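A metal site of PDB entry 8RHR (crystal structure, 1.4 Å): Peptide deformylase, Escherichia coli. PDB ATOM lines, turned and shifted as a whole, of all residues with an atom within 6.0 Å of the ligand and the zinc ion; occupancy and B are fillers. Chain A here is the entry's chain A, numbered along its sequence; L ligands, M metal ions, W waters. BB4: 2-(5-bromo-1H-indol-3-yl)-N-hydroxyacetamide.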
ATOM      1  N   GLU A  45      16.172  28.293 -15.802  1.00  0.00           N
ATOM      2  CA  GLU A  45      17.477  28.762 -15.358  1.00  0.00           C
ATOM      3  C   GLU A  45      17.780  28.368 -13.917  1.00  0.00           C
ATOM      4  O   GLU A  45      18.500  29.094 -13.229  1.00  0.00           O
ATOM      5  CB  GLU A  45      17.676  30.272 -15.600  1.00  0.00           C
ATOM      6  CG  GLU A  45      17.543  30.755 -17.063  1.00  0.00           C
ATOM      7  CD  GLU A  45      18.571  30.178 -18.116  1.00  0.00           C
ATOM      8  OE1 GLU A  45      19.618  29.604 -17.749  1.00  0.00           O
ATOM      9  OE2 GLU A  45      18.360  30.406 -19.353  1.00  0.00           O
ATOM     10  N   GLY A  46      17.241  27.189 -13.488  1.00  0.00           N
ATOM     11  CA  GLY A  46      17.501  26.610 -12.186  1.00  0.00           C
ATOM     12  C   GLY A  46      18.667  25.629 -12.173  1.00  0.00           C
ATOM     13  O   GLY A  46      19.124  25.146 -13.221  1.00  0.00           O
ATOM     14  N   ILE A  47      19.094  25.277 -10.957  1.00  0.00           N
ATOM     15  CA  ILE A  47      20.152  24.292 -10.759  1.00  0.00           C
ATOM     16  C   ILE A  47      19.626  22.990 -10.168  1.00  0.00           C
ATOM     17  O   ILE A  47      20.382  22.008 -10.076  1.00  0.00           O
ATOM     18  CB  ILE A  47      21.289  24.835  -9.859  1.00  0.00           C
ATOM     19  CG1 ILE A  47      20.724  25.251  -8.483  1.00  0.00           C
ATOM     20  CG2 ILE A  47      21.978  26.020 -10.596  1.00  0.00           C
ATOM     21  CD1 ILE A  47      21.768  25.456  -7.421  1.00  0.00           C
ATOM     22  N   GLY A  48      18.362  22.943  -9.811  1.00  0.00           N
ATOM     23  CA  GLY A  48      17.753  21.709  -9.339  1.00  0.00           C
ATOM     24  C   GLY A  48      16.259  21.777  -9.517  1.00  0.00           C
ATOM     25  O   GLY A  48      15.667  22.860  -9.613  1.00  0.00           O
ATOM     26  N   LEU A  49      15.650  20.598  -9.549  1.00  0.00           N
ATOM     27  CA  LEU A  49      14.176  20.511  -9.592  1.00  0.00           C
ATOM     28  C   LEU A  49      13.753  19.193  -8.996  1.00  0.00           C
ATOM     29  O   LEU A  49      14.320  18.149  -9.337  1.00  0.00           O
ATOM     30  CB  LEU A  49      13.676  20.624 -11.050  1.00  0.00           C
ATOM     31  CG  LEU A  49      12.203  20.828 -11.304  1.00  0.00           C
ATOM     32  CD1 LEU A  49      11.723  22.179 -10.753  1.00  0.00           C
ATOM     33  CD2 LEU A  49      11.828  20.722 -12.777  1.00  0.00           C
ATOM     34  N   ALA A  50      12.761  19.236  -8.136  1.00  0.00           N
ATOM     35  CA  ALA A  50      12.162  18.049  -7.536  1.00  0.00           C
ATOM     36  C   ALA A  50      10.813  17.793  -8.192  1.00  0.00           C
ATOM     37  O   ALA A  50      10.091  18.728  -8.566  1.00  0.00           O
ATOM     38  CB  ALA A  50      12.011  18.218  -6.008  1.00  0.00           C
ATOM     39  N   GLN A  53       7.741  19.782  -7.353  1.00  0.00           N
ATOM     40  CA  GLN A  53       7.575  21.129  -7.871  1.00  0.00           C
ATOM     41  C   GLN A  53       6.821  21.154  -9.188  1.00  0.00           C
ATOM     42  O   GLN A  53       6.335  22.215  -9.585  1.00  0.00           O
ATOM     43  CB  GLN A  53       8.941  21.792  -8.057  1.00  0.00           C
ATOM     44  CG  GLN A  53       9.714  22.095  -6.757  1.00  0.00           C
ATOM     45  CD  GLN A  53      11.049  22.683  -7.075  1.00  0.00           C
ATOM     46  OE1 GLN A  53      12.038  21.962  -7.282  1.00  0.00           O
ATOM     47  NE2 GLN A  53      11.096  23.997  -7.208  1.00  0.00           N
ATOM     48  N   ILE A  89      24.011  29.402   2.391  1.00  0.00           N
ATOM     49  CA  ILE A  89      24.017  30.463   1.413  1.00  0.00           C
ATOM     50  C   ILE A  89      22.604  31.045   1.364  1.00  0.00           C
ATOM     51  O   ILE A  89      21.670  30.466   1.897  1.00  0.00           O
ATOM     52  CB  ILE A  89      24.418  29.945   0.009  1.00  0.00           C
ATOM     53  CG1 ILE A  89      23.389  28.962  -0.556  1.00  0.00           C
ATOM     54  CG2 ILE A  89      25.868  29.441   0.054  1.00  0.00           C
ATOM     55  CD1 ILE A  89      23.659  28.508  -2.032  1.00  0.00           C
ATOM     56  N   GLU A  90      22.459  32.171   0.668  1.00  0.00           N
ATOM     57  CA  GLU A  90      21.146  32.765   0.398  1.00  0.00           C
ATOM     58  C   GLU A  90      20.504  31.980  -0.757  1.00  0.00           C
ATOM     59  O   GLU A  90      20.754  32.213  -1.951  1.00  0.00           O
ATOM     60  CB  GLU A  90      21.281  34.246   0.093  1.00  0.00           C
ATOM     61  CG  GLU A  90      21.773  35.072   1.288  1.00  0.00           C
ATOM     62  CD  GLU A  90      21.673  36.572   1.080  1.00  0.00           C
ATOM     63  OE1 GLU A  90      21.373  37.012  -0.034  1.00  0.00           O
ATOM     64  OE2 GLU A  90      21.862  37.293   2.039  1.00  0.00           O
ATOM     65  N   GLU A  91      19.708  30.982  -0.390  1.00  0.00           N
ATOM     66  CA  GLU A  91      19.066  30.097  -1.346  1.00  0.00           C
ATOM     67  C   GLU A  91      17.884  30.785  -1.981  1.00  0.00           C
ATOM     68  O   GLU A  91      17.212  31.619  -1.364  1.00  0.00           O
ATOM     69  CB  GLU A  91      18.562  28.840  -0.634  1.00  0.00           C
ATOM     70  CG  GLU A  91      19.679  27.951  -0.082  1.00  0.00           C
ATOM     71  CD  GLU A  91      19.195  26.656   0.512  1.00  0.00           C
ATOM     72  OE1 GLU A  91      18.092  26.172   0.182  1.00  0.00           O
ATOM     73  OE2 GLU A  91      19.909  26.128   1.374  1.00  0.00           O
ATOM     74  N   GLY A  92      17.641  30.403  -3.227  1.00  0.00           N
ATOM     75  CA  GLY A  92      16.414  30.719  -3.925  1.00  0.00           C
ATOM     76  C   GLY A  92      15.682  29.449  -4.279  1.00  0.00           C
ATOM     77  O   GLY A  92      16.083  28.354  -3.857  1.00  0.00           O
ATOM     78  N   CYS A  93      14.588  29.573  -5.044  1.00  0.00           N
ATOM     79  CA  CYS A  93      13.782  28.409  -5.389  1.00  0.00           C
ATOM     80  C   CYS A  93      12.886  28.833  -6.531  1.00  0.00           C
ATOM     81  O   CYS A  93      12.245  29.879  -6.428  1.00  0.00           O
ATOM     82  CB  CYS A  93      12.923  27.939  -4.212  1.00  0.00           C
ATOM     83  SG  CYS A  93      12.021  26.380  -4.541  1.00  0.00           S
ATOM     84  N   LEU A  94      12.804  28.011  -7.562  1.00  0.00           N
ATOM     85  CA  LEU A  94      11.880  28.288  -8.670  1.00  0.00           C
ATOM     86  C   LEU A  94      10.439  28.398  -8.185  1.00  0.00           C
ATOM     87  O   LEU A  94       9.630  29.054  -8.824  1.00  0.00           O
ATOM     88  CB  LEU A  94      11.984  27.220  -9.777  1.00  0.00           C
ATOM     89  CG  LEU A  94      13.291  27.184 -10.538  1.00  0.00           C
ATOM     90  CD1 LEU A  94      13.315  25.977 -11.525  1.00  0.00           C
ATOM     91  CD2 LEU A  94      13.584  28.501 -11.307  1.00  0.00           C
ATOM     92  N   SER A  95      10.092  27.734  -7.068  1.00  0.00           N
ATOM     93  CA  SER A  95       8.730  27.782  -6.540  1.00  0.00           C
ATOM     94  C   SER A  95       8.503  28.977  -5.613  1.00  0.00           C
ATOM     95  O   SER A  95       7.375  29.179  -5.130  1.00  0.00           O
ATOM     96  CB  SER A  95       8.372  26.488  -5.795  1.00  0.00           C
ATOM     97  OG  SER A  95       8.447  25.337  -6.619  1.00  0.00           O
ATOM     98  N   LEU A 128      28.246  23.853  -2.836  1.00  0.00           N
ATOM     99  CA  LEU A 128      26.949  24.139  -3.428  1.00  0.00           C
ATOM    100  C   LEU A 128      26.190  22.853  -3.738  1.00  0.00           C
ATOM    101  O   LEU A 128      24.973  22.794  -3.544  1.00  0.00           O
ATOM    102  CB  LEU A 128      27.143  24.974  -4.695  1.00  0.00           C
ATOM    103  CG  LEU A 128      25.917  25.263  -5.518  1.00  0.00           C
ATOM    104  CD1 LEU A 128      24.982  26.151  -4.753  1.00  0.00           C
ATOM    105  CD2 LEU A 128      26.282  25.955  -6.832  1.00  0.00           C
ATOM    106  N   ILE A 131      24.428  21.551  -0.702  1.00  0.00           N
ATOM    107  CA  ILE A 131      23.284  22.420  -0.338  1.00  0.00           C
ATOM    108  C   ILE A 131      22.109  22.128  -1.281  1.00  0.00           C
ATOM    109  O   ILE A 131      20.959  21.948  -0.842  1.00  0.00           O
ATOM    110  CB  ILE A 131      23.718  23.885  -0.410  1.00  0.00           C
ATOM    111  CG1 ILE A 131      24.669  24.201   0.750  1.00  0.00           C
ATOM    112  CG2 ILE A 131      22.501  24.798  -0.436  1.00  0.00           C
ATOM    113  CD1 ILE A 131      25.395  25.484   0.581  1.00  0.00           C
ATOM    114  N   CYS A 132      22.392  22.023  -2.576  1.00  0.00           N
ATOM    115  CA  CYS A 132      21.320  21.765  -3.537  1.00  0.00           C
ATOM    116  C   CYS A 132      20.664  20.379  -3.337  1.00  0.00           C
ATOM    117  O   CYS A 132      19.428  20.260  -3.368  1.00  0.00           O
ATOM    118  CB  CYS A 132      21.931  21.927  -4.918  1.00  0.00           C
ATOM    119  SG  CYS A 132      20.748  21.756  -6.244  1.00  0.00           S
ATOM    120  N   HIS A 135      18.343  20.804  -0.326  1.00  0.00           N
ATOM    121  CA  HIS A 135      17.177  21.592  -0.749  1.00  0.00           C
ATOM    122  C   HIS A 135      16.202  20.754  -1.571  1.00  0.00           C
ATOM    123  O   HIS A 135      14.994  20.758  -1.304  1.00  0.00           O
ATOM    124  CB  HIS A 135      17.704  22.816  -1.504  1.00  0.00           C
ATOM    125  CG  HIS A 135      16.643  23.691  -2.067  1.00  0.00           C
ATOM    126  ND1 HIS A 135      16.580  25.043  -1.795  1.00  0.00           N
ATOM    127  CD2 HIS A 135      15.706  23.455  -3.015  1.00  0.00           C
ATOM    128  CE1 HIS A 135      15.614  25.594  -2.513  1.00  0.00           C
ATOM    129  NE2 HIS A 135      15.048  24.656  -3.238  1.00  0.00           N
ATOM    130  N   GLU A 136      16.718  20.000  -2.546  1.00  0.00           N
ATOM    131  CA  GLU A 136      15.839  19.215  -3.391  1.00  0.00           C
ATOM    132  C   GLU A 136      15.228  18.036  -2.638  1.00  0.00           C
ATOM    133  O   GLU A 136      14.054  17.724  -2.835  1.00  0.00           O
ATOM    134  CB  GLU A 136      16.569  18.784  -4.666  1.00  0.00           C
ATOM    135  CG  GLU A 136      17.090  19.923  -5.501  1.00  0.00           C
ATOM    136  CD  GLU A 136      16.119  20.984  -5.876  1.00  0.00           C
ATOM    137  OE1 GLU A 136      14.933  20.680  -5.919  1.00  0.00           O
ATOM    138  OE2 GLU A 136      16.568  22.159  -6.113  1.00  0.00           O
ATOM    139  N   HIS A 139      12.197  19.173  -0.809  1.00  0.00           N
ATOM    140  CA  HIS A 139      10.989  19.292  -1.612  1.00  0.00           C
ATOM    141  C   HIS A 139      10.208  17.993  -1.621  1.00  0.00           C
ATOM    142  O   HIS A 139       8.983  18.005  -1.605  1.00  0.00           O
ATOM    143  CB  HIS A 139      11.313  19.678  -3.056  1.00  0.00           C
ATOM    144  CG  HIS A 139      11.529  21.136  -3.321  1.00  0.00           C
ATOM    145  ND1 HIS A 139      10.565  22.079  -3.069  1.00  0.00           N
ATOM    146  CD2 HIS A 139      12.554  21.797  -3.924  1.00  0.00           C
ATOM    147  CE1 HIS A 139      10.977  23.268  -3.469  1.00  0.00           C
ATOM    148  NE2 HIS A 139      12.195  23.140  -3.957  1.00  0.00           N
ATOM    149  N   LEU A 144      10.126  23.487   2.240  1.00  0.00           N
ATOM    150  CA  LEU A 144      10.623  24.599   1.440  1.00  0.00           C
ATOM    151  C   LEU A 144      11.654  25.374   2.244  1.00  0.00           C
ATOM    152  O   LEU A 144      11.641  25.369   3.482  1.00  0.00           O
ATOM    153  CB  LEU A 144       9.445  25.532   1.065  1.00  0.00           C
ATOM    154  CG  LEU A 144       8.296  24.877   0.307  1.00  0.00           C
ATOM    155  CD1 LEU A 144       7.159  25.890   0.185  1.00  0.00           C
ATOM    156  CD2 LEU A 144       8.800  24.405  -1.054  1.00  0.00           C
ATOM    157  N   PHE A 145      12.533  26.108   1.553  1.00  0.00           N
ATOM    158  CA  PHE A 145      13.617  26.745   2.279  1.00  0.00           C
ATOM    159  C   PHE A 145      13.108  27.770   3.268  1.00  0.00           C
ATOM    160  O   PHE A 145      13.719  28.000   4.326  1.00  0.00           O
ATOM    161  CB  PHE A 145      14.698  27.336   1.361  1.00  0.00           C
ATOM    162  CG  PHE A 145      14.348  28.669   0.759  1.00  0.00           C
ATOM    163  CD1 PHE A 145      14.457  29.854   1.486  1.00  0.00           C
ATOM    164  CD2 PHE A 145      13.975  28.751  -0.578  1.00  0.00           C
ATOM    165  CE1 PHE A 145      14.165  31.084   0.890  1.00  0.00           C
ATOM    166  CE2 PHE A 145      13.680  29.991  -1.165  1.00  0.00           C
ATOM    167  CZ  PHE A 145      13.775  31.147  -0.430  1.00  0.00           C
HETATM  168 BR   BB4 L   1      20.073  25.324  -3.236  1.00  0.00          BR
HETATM  169  N1  BB4 L   1      14.851  24.148  -6.254  1.00  0.00           N
HETATM  170  O2  BB4 L   1      13.860  25.417  -7.841  1.00  0.00           O
HETATM  171  N3  BB4 L   1      17.472  28.650  -7.364  1.00  0.00           N
HETATM  172  C4  BB4 L   1      16.691  27.720  -7.995  1.00  0.00           C
HETATM  173  C5  BB4 L   1      16.867  26.507  -7.398  1.00  0.00           C
HETATM  174  C6  BB4 L   1      17.813  26.699  -6.327  1.00  0.00           C
HETATM  175  C7  BB4 L   1      18.390  25.862  -5.384  1.00  0.00           C
HETATM  176  C8  BB4 L   1      19.283  26.447  -4.509  1.00  0.00           C
HETATM  177  C9  BB4 L   1      19.676  27.778  -4.510  1.00  0.00           C
HETATM  178  C10 BB4 L   1      19.121  28.614  -5.457  1.00  0.00           C
HETATM  179  C11 BB4 L   1      18.171  28.071  -6.344  1.00  0.00           C
HETATM  180  C12 BB4 L   1      16.229  25.222  -7.751  1.00  0.00           C
HETATM  181  C13 BB4 L   1      14.830  24.997  -7.301  1.00  0.00           C
HETATM  182  O14 BB4 L   1      13.795  23.354  -5.939  1.00  0.00           O
HETATM  183 ZN    ZN M   1      13.444  24.659  -4.586  1.00  0.00          ZN
HETATM  184  O   HOH W   1      16.660  30.556  -9.987  1.00  0.00           O
HETATM  185  O   HOH W   2      17.968  31.724  -7.309  1.00  0.00           O
HETATM  186  O   HOH W   3      21.268  30.887  -4.276  1.00  0.00           O
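Ile 47 touches the ligand (CG1 to C6, 3.9 Å). O of Gly 48 touches C12 of the ligand (3.1 Å). Glu 91 touches the ligand (CA to C9, 3.97 Å). Gly 92 touches the ligand. Ile 131 touches the ligand (CG2 to BR, 3.7 Å). Cys 132 touches the ligand (CA to BR, 3.8 Å). Hydrophobic or aromatic side chains within 4 Å of the ligand: Ile 47, Leu 94, Ile 131, His 135 and His 139. 12 residues have an atom within 4 Å of the ligand: Ile 47, Gly 48, Gln 53, Glu 91, Gly 92, Cys 93, Leu 94, Ile 131, Cys 132, His 135, Glu 136 and His 139. The nearest printed residue that does not touch the ligand is Gly 46 (4.4 Å).
Gln 53 touches the zinc ion (NE2 to ZN, 3.6 Å). Within 4 Å of the zinc ion: Gln 53, Cys 93, His 135 and His 139.
The zinc ion is bound by an oxygen (O14) of the ligand (1.9 Å), a ring nitrogen (NE2) of His 139 (2.1 Å), a ring nitrogen (NE2) of His 135 (2.1 Å) and the side-chain sulfur (SG) of Cys 93 (2.2 Å).
OE1 of Gln 53 sits at hydrogen-bond distance from N of Ala 50. N of Ala 50 is in hydrogen-bond range of OE1 of Glu 136 (3.4 Å). NE2 of Gln 53 sits at hydrogen-bond distance from OG of Ser 95 (3.0 Å). The side-chain sulfur (SG) of Cys 93 lies close to the side-chain amide nitrogen (NE2) of Gln 53, at 3.7 Å. SG of Cys 93 sits close to N of Ser 95. The side-chain carboxylate (OE1) of Glu 136 sits close to the side-chain amide oxygen (OE1) of Gln 53, at 3.4 Å. The side-chain carboxylate of Glu 91 lies within hydrogen-bond range of a ring nitrogen (ND1) of His 135, at 2.7 Å.
NE2 of Gln 53 lies within hydrogen-bond range of O2 of the ligand (3.2 Å). The backbone NH (N) of Leu 94 lies within hydrogen-bond range of an oxygen (O2) of the ligand (2.8 Å). N1 of the ligand lies close to OE2 of Glu 136 (2.6 Å).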
